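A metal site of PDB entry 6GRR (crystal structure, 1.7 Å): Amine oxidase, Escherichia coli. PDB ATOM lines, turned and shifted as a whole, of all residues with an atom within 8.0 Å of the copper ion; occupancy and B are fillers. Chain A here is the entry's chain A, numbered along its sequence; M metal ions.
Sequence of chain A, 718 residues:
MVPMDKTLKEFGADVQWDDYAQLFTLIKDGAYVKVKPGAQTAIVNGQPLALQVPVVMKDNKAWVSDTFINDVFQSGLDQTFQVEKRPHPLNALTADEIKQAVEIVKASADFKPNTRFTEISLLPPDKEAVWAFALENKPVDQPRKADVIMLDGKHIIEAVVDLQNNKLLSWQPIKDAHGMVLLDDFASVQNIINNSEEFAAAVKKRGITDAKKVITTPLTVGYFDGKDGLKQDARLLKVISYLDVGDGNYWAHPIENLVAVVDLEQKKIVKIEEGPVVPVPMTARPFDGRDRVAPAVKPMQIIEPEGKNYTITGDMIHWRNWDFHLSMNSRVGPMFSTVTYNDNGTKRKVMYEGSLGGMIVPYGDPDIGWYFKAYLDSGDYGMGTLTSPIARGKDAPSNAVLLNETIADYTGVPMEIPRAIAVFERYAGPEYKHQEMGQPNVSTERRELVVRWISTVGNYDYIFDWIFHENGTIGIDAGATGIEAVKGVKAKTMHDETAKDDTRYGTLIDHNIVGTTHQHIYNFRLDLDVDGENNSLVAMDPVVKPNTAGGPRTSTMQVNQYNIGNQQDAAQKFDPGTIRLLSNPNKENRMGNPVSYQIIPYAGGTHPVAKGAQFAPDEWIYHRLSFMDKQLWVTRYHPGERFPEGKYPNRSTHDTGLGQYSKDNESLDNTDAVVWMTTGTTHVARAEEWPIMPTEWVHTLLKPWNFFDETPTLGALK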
ATOM      1  N   VAL A 361      17.930 -11.559  14.586  1.00  0.00           N
ATOM      2  CA  VAL A 361      18.740 -12.793  14.554  1.00  0.00           C
ATOM      3  C   VAL A 361      18.633 -13.338  13.113  1.00  0.00           C
ATOM      4  O   VAL A 361      17.717 -14.092  12.811  1.00  0.00           O
ATOM      5  CB  VAL A 361      18.206 -13.802  15.542  1.00  0.00           C
ATOM      6  CG1 VAL A 361      19.063 -15.068  15.538  1.00  0.00           C
ATOM      7  CG2 VAL A 361      18.174 -13.183  16.927  1.00  0.00           C
ATOM      8  N   TYR A 363      20.091 -15.352   9.636  1.00  0.00           N
ATOM      9  CA  TYR A 363      20.874 -16.534   9.339  1.00  0.00           C
ATOM     10  C   TYR A 363      21.712 -16.419   8.059  1.00  0.00           C
ATOM     11  O   TYR A 363      21.483 -15.542   7.226  1.00  0.00           O
ATOM     12  CB  TYR A 363      19.967 -17.752   9.328  1.00  0.00           C
ATOM     13  CG  TYR A 363      19.570 -18.132  10.755  1.00  0.00           C
ATOM     14  CD1 TYR A 363      18.640 -17.375  11.461  1.00  0.00           C
ATOM     15  CD2 TYR A 363      20.204 -19.192  11.405  1.00  0.00           C
ATOM     16  CE1 TYR A 363      18.304 -17.697  12.791  1.00  0.00           C
ATOM     17  CE2 TYR A 363      19.888 -19.515  12.721  1.00  0.00           C
ATOM     18  CZ  TYR A 363      18.953 -18.755  13.397  1.00  0.00           C
ATOM     19  OH  TYR A 363      18.666 -19.078  14.697  1.00  0.00           O
ATOM     20  N   ASN A 459      12.492 -20.489  19.852  1.00  0.00           N
ATOM     21  CA  ASN A 459      13.572 -21.370  20.323  1.00  0.00           C
ATOM     22  C   ASN A 459      14.547 -20.684  21.273  1.00  0.00           C
ATOM     23  O   ASN A 459      15.102 -21.332  22.152  1.00  0.00           O
ATOM     24  CB  ASN A 459      14.352 -21.992  19.151  1.00  0.00           C
ATOM     25  CG  ASN A 459      14.874 -20.976  18.166  1.00  0.00           C
ATOM     26  OD1 ASN A 459      14.079 -20.233  17.591  1.00  0.00           O
ATOM     27  ND2 ASN A 459      16.196 -20.911  17.976  1.00  0.00           N
ATOM     28  N   TYR A 460      14.739 -19.386  21.105  1.00  0.00           N
ATOM     29  CA  TYR A 460      15.757 -18.679  21.895  1.00  0.00           C
ATOM     30  C   TYR A 460      15.125 -17.871  23.051  1.00  0.00           C
ATOM     31  O   TYR A 460      13.998 -17.386  22.931  1.00  0.00           O
ATOM     32  CB  TYR A 460      16.573 -17.731  21.019  1.00  0.00           C
ATOM     33  CG  TYR A 460      17.819 -18.302  20.346  1.00  0.00           C
ATOM     34  CD1 TYR A 460      18.802 -18.963  21.078  1.00  0.00           C
ATOM     35  CD2 TYR A 460      18.036 -18.117  18.991  1.00  0.00           C
ATOM     36  CE1 TYR A 460      19.974 -19.441  20.472  1.00  0.00           C
ATOM     37  CE2 TYR A 460      19.209 -18.604  18.373  1.00  0.00           C
ATOM     38  CZ  TYR A 460      20.180 -19.250  19.120  1.00  0.00           C
ATOM     39  OH  TYR A 460      21.343 -19.724  18.537  1.00  0.00           O
ATOM     40  N   TYR A 462      16.078 -14.656  25.698  1.00  0.00           N
ATOM     41  CA  TYR A 462      16.928 -13.498  25.826  1.00  0.00           C
ATOM     42  C   TYR A 462      16.747 -12.881  27.209  1.00  0.00           C
ATOM     43  O   TYR A 462      15.616 -12.749  27.683  1.00  0.00           O
ATOM     44  CB  TYR A 462      16.612 -12.483  24.728  1.00  0.00           C
ATOM     45  CG  TYR A 462      16.875 -13.056  23.355  1.00  0.00           C
ATOM     46  CD1 TYR A 462      18.191 -13.261  22.949  1.00  0.00           C
ATOM     47  CD2 TYR A 462      15.833 -13.454  22.516  1.00  0.00           C
ATOM     48  CE1 TYR A 462      18.479 -13.834  21.734  1.00  0.00           C
ATOM     49  CE2 TYR A 462      16.111 -14.037  21.282  1.00  0.00           C
ATOM     50  CZ  TYR A 462      17.440 -14.210  20.897  1.00  0.00           C
ATOM     51  OH  TYR A 462      17.781 -14.802  19.701  1.00  0.00           O
ATOM     52  N   ALA A 480      21.911 -14.656  25.939  1.00  0.00           N
ATOM     53  CA  ALA A 480      21.112 -15.515  25.067  1.00  0.00           C
ATOM     54  C   ALA A 480      21.318 -16.954  25.509  1.00  0.00           C
ATOM     55  O   ALA A 480      22.447 -17.356  25.813  1.00  0.00           O
ATOM     56  CB  ALA A 480      21.508 -15.342  23.604  1.00  0.00           C
ATOM     57  N   THR A 481      20.213 -17.681  25.617  1.00  0.00           N
ATOM     58  CA  THR A 481      20.200 -19.099  25.929  1.00  0.00           C
ATOM     59  C   THR A 481      19.038 -19.716  25.158  1.00  0.00           C
ATOM     60  O   THR A 481      18.454 -19.068  24.295  1.00  0.00           O
ATOM     61  CB  THR A 481      20.199 -19.343  27.449  1.00  0.00           C
ATOM     62  OG1 THR A 481      20.254 -20.765  27.717  1.00  0.00           O
ATOM     63  CG2 THR A 481      19.004 -18.728  28.138  1.00  0.00           C
ATOM     64  N   ILE A 483      17.430 -22.911  22.653  1.00  0.00           N
ATOM     65  CA  ILE A 483      17.672 -24.056  21.768  1.00  0.00           C
ATOM     66  C   ILE A 483      18.061 -23.498  20.395  1.00  0.00           C
ATOM     67  O   ILE A 483      17.359 -22.661  19.865  1.00  0.00           O
ATOM     68  CB  ILE A 483      16.416 -24.938  21.600  1.00  0.00           C
ATOM     69  CG1 ILE A 483      15.721 -25.225  22.953  1.00  0.00           C
ATOM     70  CG2 ILE A 483      16.778 -26.253  20.917  1.00  0.00           C
ATOM     71  CD1 ILE A 483      16.553 -25.925  23.998  1.00  0.00           C
ATOM     72  N   GLU A 484      19.171 -23.961  19.833  1.00  0.00           N
ATOM     73  CA  GLU A 484      19.596 -23.526  18.499  1.00  0.00           C
ATOM     74  C   GLU A 484      18.662 -23.983  17.406  1.00  0.00           C
ATOM     75  O   GLU A 484      18.028 -25.027  17.537  1.00  0.00           O
ATOM     76  CB  GLU A 484      21.023 -23.968  18.237  1.00  0.00           C
ATOM     77  CG  GLU A 484      21.989 -23.205  19.157  1.00  0.00           C
ATOM     78  CD  GLU A 484      23.431 -23.561  18.974  1.00  0.00           C
ATOM     79  OE1 GLU A 484      23.776 -24.400  18.096  1.00  0.00           O
ATOM     80  OE2 GLU A 484      24.245 -23.011  19.764  1.00  0.00           O
ATOM     81  N   ALA A 485      18.522 -23.149  16.375  1.00  0.00           N
ATOM     82  CA  ALA A 485      17.798 -23.498  15.151  1.00  0.00           C
ATOM     83  C   ALA A 485      18.754 -24.298  14.322  1.00  0.00           C
ATOM     84  O   ALA A 485      19.835 -23.785  13.946  1.00  0.00           O
ATOM     85  CB  ALA A 485      17.383 -22.255  14.388  1.00  0.00           C
ATOM     86  N   THR A 516      23.285 -23.854  12.214  1.00  0.00           N
ATOM     87  CA  THR A 516      23.500 -22.885  11.150  1.00  0.00           C
ATOM     88  C   THR A 516      24.018 -21.555  11.703  1.00  0.00           C
ATOM     89  O   THR A 516      23.445 -21.021  12.650  1.00  0.00           O
ATOM     90  CB  THR A 516      22.213 -22.655  10.353  1.00  0.00           C
ATOM     91  OG1 THR A 516      21.735 -23.927   9.841  1.00  0.00           O
ATOM     92  CG2 THR A 516      22.425 -21.667   9.241  1.00  0.00           C
ATOM     93  N   THR A 517      25.064 -21.019  11.081  1.00  0.00           N
ATOM     94  CA  THR A 517      25.675 -19.774  11.502  1.00  0.00           C
ATOM     95  C   THR A 517      24.705 -18.613  11.310  1.00  0.00           C
ATOM     96  O   THR A 517      23.911 -18.564  10.353  1.00  0.00           O
ATOM     97  CB  THR A 517      27.022 -19.528  10.765  1.00  0.00           C
ATOM     98  OG1 THR A 517      27.916 -20.596  11.075  1.00  0.00           O
ATOM     99  CG2 THR A 517      27.681 -18.221  11.215  1.00  0.00           C
ATOM    100  N   HIS A 518      24.759 -17.687  12.264  1.00  0.00           N
ATOM    101  CA  HIS A 518      23.867 -16.538  12.271  1.00  0.00           C
ATOM    102  C   HIS A 518      24.447 -15.478  13.189  1.00  0.00           C
ATOM    103  O   HIS A 518      25.492 -15.690  13.769  1.00  0.00           O
ATOM    104  CB  HIS A 518      22.502 -16.970  12.774  1.00  0.00           C
ATOM    105  CG  HIS A 518      22.563 -17.618  14.110  1.00  0.00           C
ATOM    106  ND1 HIS A 518      22.990 -18.919  14.278  1.00  0.00           N
ATOM    107  CD2 HIS A 518      22.324 -17.119  15.346  1.00  0.00           C
ATOM    108  CE1 HIS A 518      22.988 -19.206  15.568  1.00  0.00           C
ATOM    109  NE2 HIS A 518      22.582 -18.124  16.230  1.00  0.00           N
ATOM    110  N   GLN A 519      23.764 -14.329  13.309  1.00  0.00           N
ATOM    111  CA  GLN A 519      24.178 -13.303  14.256  1.00  0.00           C
ATOM    112  C   GLN A 519      23.080 -13.086  15.257  1.00  0.00           C
ATOM    113  O   GLN A 519      21.919 -13.378  14.978  1.00  0.00           O
ATOM    114  CB  GLN A 519      24.473 -11.984  13.558  1.00  0.00           C
ATOM    115  CG  GLN A 519      25.612 -12.102  12.550  1.00  0.00           C
ATOM    116  CD  GLN A 519      25.927 -10.787  11.910  1.00  0.00           C
ATOM    117  OE1 GLN A 519      25.255 -10.355  10.975  1.00  0.00           O
ATOM    118  NE2 GLN A 519      26.952 -10.134  12.424  1.00  0.00           N
ATOM    119  N   HIS A 520      23.448 -12.583  16.437  1.00  0.00           N
ATOM    120  CA  HIS A 520      22.472 -11.974  17.349  1.00  0.00           C
ATOM    121  C   HIS A 520      22.815 -10.504  17.419  1.00  0.00           C
ATOM    122  O   HIS A 520      23.932 -10.160  17.806  1.00  0.00           O
ATOM    123  CB  HIS A 520      22.544 -12.589  18.758  1.00  0.00           C
ATOM    124  CG  HIS A 520      22.206 -14.056  18.790  1.00  0.00           C
ATOM    125  ND1 HIS A 520      20.947 -14.523  19.083  1.00  0.00           N
ATOM    126  CD2 HIS A 520      22.971 -15.143  18.580  1.00  0.00           C
ATOM    127  CE1 HIS A 520      20.955 -15.842  19.054  1.00  0.00           C
ATOM    128  NE2 HIS A 520      22.179 -16.241  18.745  1.00  0.00           N
ATOM    129  N   TYR A 522      21.523  -6.727  18.820  1.00  0.00           N
ATOM    130  CA  TYR A 522      20.630  -5.993  19.711  1.00  0.00           C
ATOM    131  C   TYR A 522      20.858  -4.497  19.509  1.00  0.00           C
ATOM    132  O   TYR A 522      21.967  -4.082  19.311  1.00  0.00           O
ATOM    133  CB  TYR A 522      20.928  -6.297  21.185  1.00  0.00           C
ATOM    134  CG  TYR A 522      21.069  -7.763  21.492  1.00  0.00           C
ATOM    135  CD1 TYR A 522      19.957  -8.530  21.812  1.00  0.00           C
ATOM    136  CD2 TYR A 522      22.294  -8.376  21.485  1.00  0.00           C
ATOM    137  CE1 TYR A 522      20.069  -9.893  22.086  1.00  0.00           C
ATOM    138  CE2 TYR A 522      22.428  -9.742  21.755  1.00  0.00           C
ATOM    139  CZ  TYR A 522      21.303 -10.478  22.060  1.00  0.00           C
ATOM    140  OH  TYR A 522      21.391 -11.829  22.341  1.00  0.00           O
ATOM    141  N   HIS A 607      30.666 -14.592  22.997  1.00  0.00           N
ATOM    142  CA  HIS A 607      30.707 -15.104  21.623  1.00  0.00           C
ATOM    143  C   HIS A 607      31.531 -14.152  20.735  1.00  0.00           C
ATOM    144  O   HIS A 607      31.773 -12.986  21.086  1.00  0.00           O
ATOM    145  CB  HIS A 607      29.297 -15.212  21.024  1.00  0.00           C
ATOM    146  CG  HIS A 607      28.622 -16.563  21.198  1.00  0.00           C
ATOM    147  ND1 HIS A 607      27.259 -16.720  21.067  1.00  0.00           N
ATOM    148  CD2 HIS A 607      29.122 -17.807  21.410  1.00  0.00           C
ATOM    149  CE1 HIS A 607      26.948 -17.996  21.208  1.00  0.00           C
ATOM    150  NE2 HIS A 607      28.052 -18.670  21.454  1.00  0.00           N
ATOM    151  N   THR A 681      26.754 -10.340  18.031  1.00  0.00           N
ATOM    152  CA  THR A 681      27.683 -11.460  17.980  1.00  0.00           C
ATOM    153  C   THR A 681      27.509 -12.196  16.662  1.00  0.00           C
ATOM    154  O   THR A 681      26.462 -12.094  16.038  1.00  0.00           O
ATOM    155  CB  THR A 681      27.403 -12.452  19.125  1.00  0.00           C
ATOM    156  OG1 THR A 681      26.096 -13.022  18.963  1.00  0.00           O
ATOM    157  CG2 THR A 681      27.488 -11.726  20.469  1.00  0.00           C
ATOM    158  N   THR A 682      28.533 -12.912  16.240  1.00  0.00           N
ATOM    159  CA  THR A 682      28.464 -13.883  15.161  1.00  0.00           C
ATOM    160  C   THR A 682      28.564 -15.248  15.837  1.00  0.00           C
ATOM    161  O   THR A 682      29.605 -15.617  16.399  1.00  0.00           O
ATOM    162  CB  THR A 682      29.604 -13.651  14.155  1.00  0.00           C
ATOM    163  OG1 THR A 682      29.364 -12.421  13.458  1.00  0.00           O
ATOM    164  CG2 THR A 682      29.668 -14.772  13.133  1.00  0.00           C
ATOM    165  N   HIS A 683      27.469 -15.977  15.799  1.00  0.00           N
ATOM    166  CA  HIS A 683      27.352 -17.213  16.513  1.00  0.00           C
ATOM    167  C   HIS A 683      27.714 -18.388  15.581  1.00  0.00           C
ATOM    168  O   HIS A 683      26.904 -18.796  14.777  1.00  0.00           O
ATOM    169  CB  HIS A 683      25.935 -17.357  17.092  1.00  0.00           C
ATOM    170  CG  HIS A 683      25.713 -18.573  17.932  1.00  0.00           C
ATOM    171  ND1 HIS A 683      24.500 -18.831  18.549  1.00  0.00           N
ATOM    172  CD2 HIS A 683      26.549 -19.573  18.293  1.00  0.00           C
ATOM    173  CE1 HIS A 683      24.598 -19.971  19.212  1.00  0.00           C
ATOM    174  NE2 HIS A 683      25.820 -20.444  19.069  1.00  0.00           N
ATOM    175  N   VAL A 684      28.919 -18.898  15.734  1.00  0.00           N
ATOM    176  CA  VAL A 684      29.336 -20.171  15.149  1.00  0.00           C
ATOM    177  C   VAL A 684      29.193 -21.210  16.251  1.00  0.00           C
ATOM    178  O   VAL A 684      29.729 -21.056  17.355  1.00  0.00           O
ATOM    179  CB  VAL A 684      30.779 -20.122  14.605  1.00  0.00           C
ATOM    180  CG1 VAL A 684      31.248 -21.479  14.101  1.00  0.00           C
ATOM    181  CG2 VAL A 684      30.890 -19.082  13.498  1.00  0.00           C
ATOM    182  N   ALA A 685      28.426 -22.249  15.957  1.00  0.00           N
ATOM    183  CA  ALA A 685      27.983 -23.209  16.943  1.00  0.00           C
ATOM    184  C   ALA A 685      29.041 -24.254  17.337  1.00  0.00           C
ATOM    185  O   ALA A 685      30.019 -24.485  16.625  1.00  0.00           O
ATOM    186  CB  ALA A 685      26.731 -23.912  16.436  1.00  0.00           C
ATOM    187  N   GLU A 689      26.825 -26.481  23.043  1.00  0.00           N
ATOM    188  CA  GLU A 689      25.595 -25.674  23.024  1.00  0.00           C
ATOM    189  C   GLU A 689      24.343 -26.474  22.649  1.00  0.00           C
ATOM    190  O   GLU A 689      23.265 -25.909  22.405  1.00  0.00           O
ATOM    191  CB  GLU A 689      25.792 -24.466  22.075  1.00  0.00           C
ATOM    192  CG  GLU A 689      26.974 -23.565  22.424  1.00  0.00           C
ATOM    193  CD  GLU A 689      27.357 -22.564  21.342  1.00  0.00           C
ATOM    194  OE1 GLU A 689      26.905 -22.696  20.142  1.00  0.00           O
ATOM    195  OE2 GLU A 689      28.125 -21.630  21.695  1.00  0.00           O
ATOM    196  N   MET A 693      21.719 -24.288  25.031  1.00  0.00           N
ATOM    197  CA  MET A 693      22.877 -23.390  24.943  1.00  0.00           C
ATOM    198  C   MET A 693      23.167 -22.713  26.262  1.00  0.00           C
ATOM    199  O   MET A 693      22.346 -21.920  26.714  1.00  0.00           O
ATOM    200  CB  MET A 693      22.652 -22.303  23.898  1.00  0.00           C
ATOM    201  CG  MET A 693      23.897 -21.433  23.760  1.00  0.00           C
ATOM    202  SD  MET A 693      23.871 -20.214  22.435  1.00  0.00           S
ATOM    203  CE  MET A 693      22.756 -18.936  22.994  1.00  0.00           C
ATOM    204  N   GLU A 696      25.112 -17.067  26.988  1.00  0.00           N
ATOM    205  CA  GLU A 696      26.209 -16.256  26.461  1.00  0.00           C
ATOM    206  C   GLU A 696      25.833 -14.788  26.631  1.00  0.00           C
ATOM    207  O   GLU A 696      24.670 -14.451  26.448  1.00  0.00           O
ATOM    208  CB  GLU A 696      26.428 -16.548  24.986  1.00  0.00           C
ATOM    209  CG  GLU A 696      26.767 -18.026  24.699  1.00  0.00           C
ATOM    210  CD  GLU A 696      28.239 -18.372  24.861  1.00  0.00           C
ATOM    211  OE1 GLU A 696      29.051 -17.496  25.311  1.00  0.00           O
ATOM    212  OE2 GLU A 696      28.593 -19.554  24.545  1.00  0.00           O
HETATM  213 CU    CU M   1      22.695 -18.094  18.244  1.00  0.00          CU
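Within 4 Å of the copper ion: Tyr 460, His 518, His 520 and His 683.
A ring nitrogen (NE2) of His 683 is in hydrogen-bond range of the side-chain carboxylate (OE2) of Glu 484, at 3.1 Å.
NE2 of His 683 sits at hydrogen-bond distance from OE1 of Glu 689 (2.7 Å).
The side-chain hydroxyl (OH) of Tyr 462 lies within hydrogen-bond range of a ring nitrogen (ND1) of His 520 (3.2 Å).
The backbone carbonyl oxygen of His 520 lies within hydrogen-bond range of the backbone NH of Thr 681, at 2.8 Å.
The backbone carbonyl oxygen of Thr 516 is in hydrogen-bond range of a ring nitrogen (ND1) of His 518 (2.7 Å).
The copper ion is bound by ND1 of His 683 (2.0 Å), NE2 of His 520 (2.0 Å), NE2 of His 518 (2.0 Å) and OH of Tyr 460 (2.1 Å).
The copper ion has four donor atoms within binding distance.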
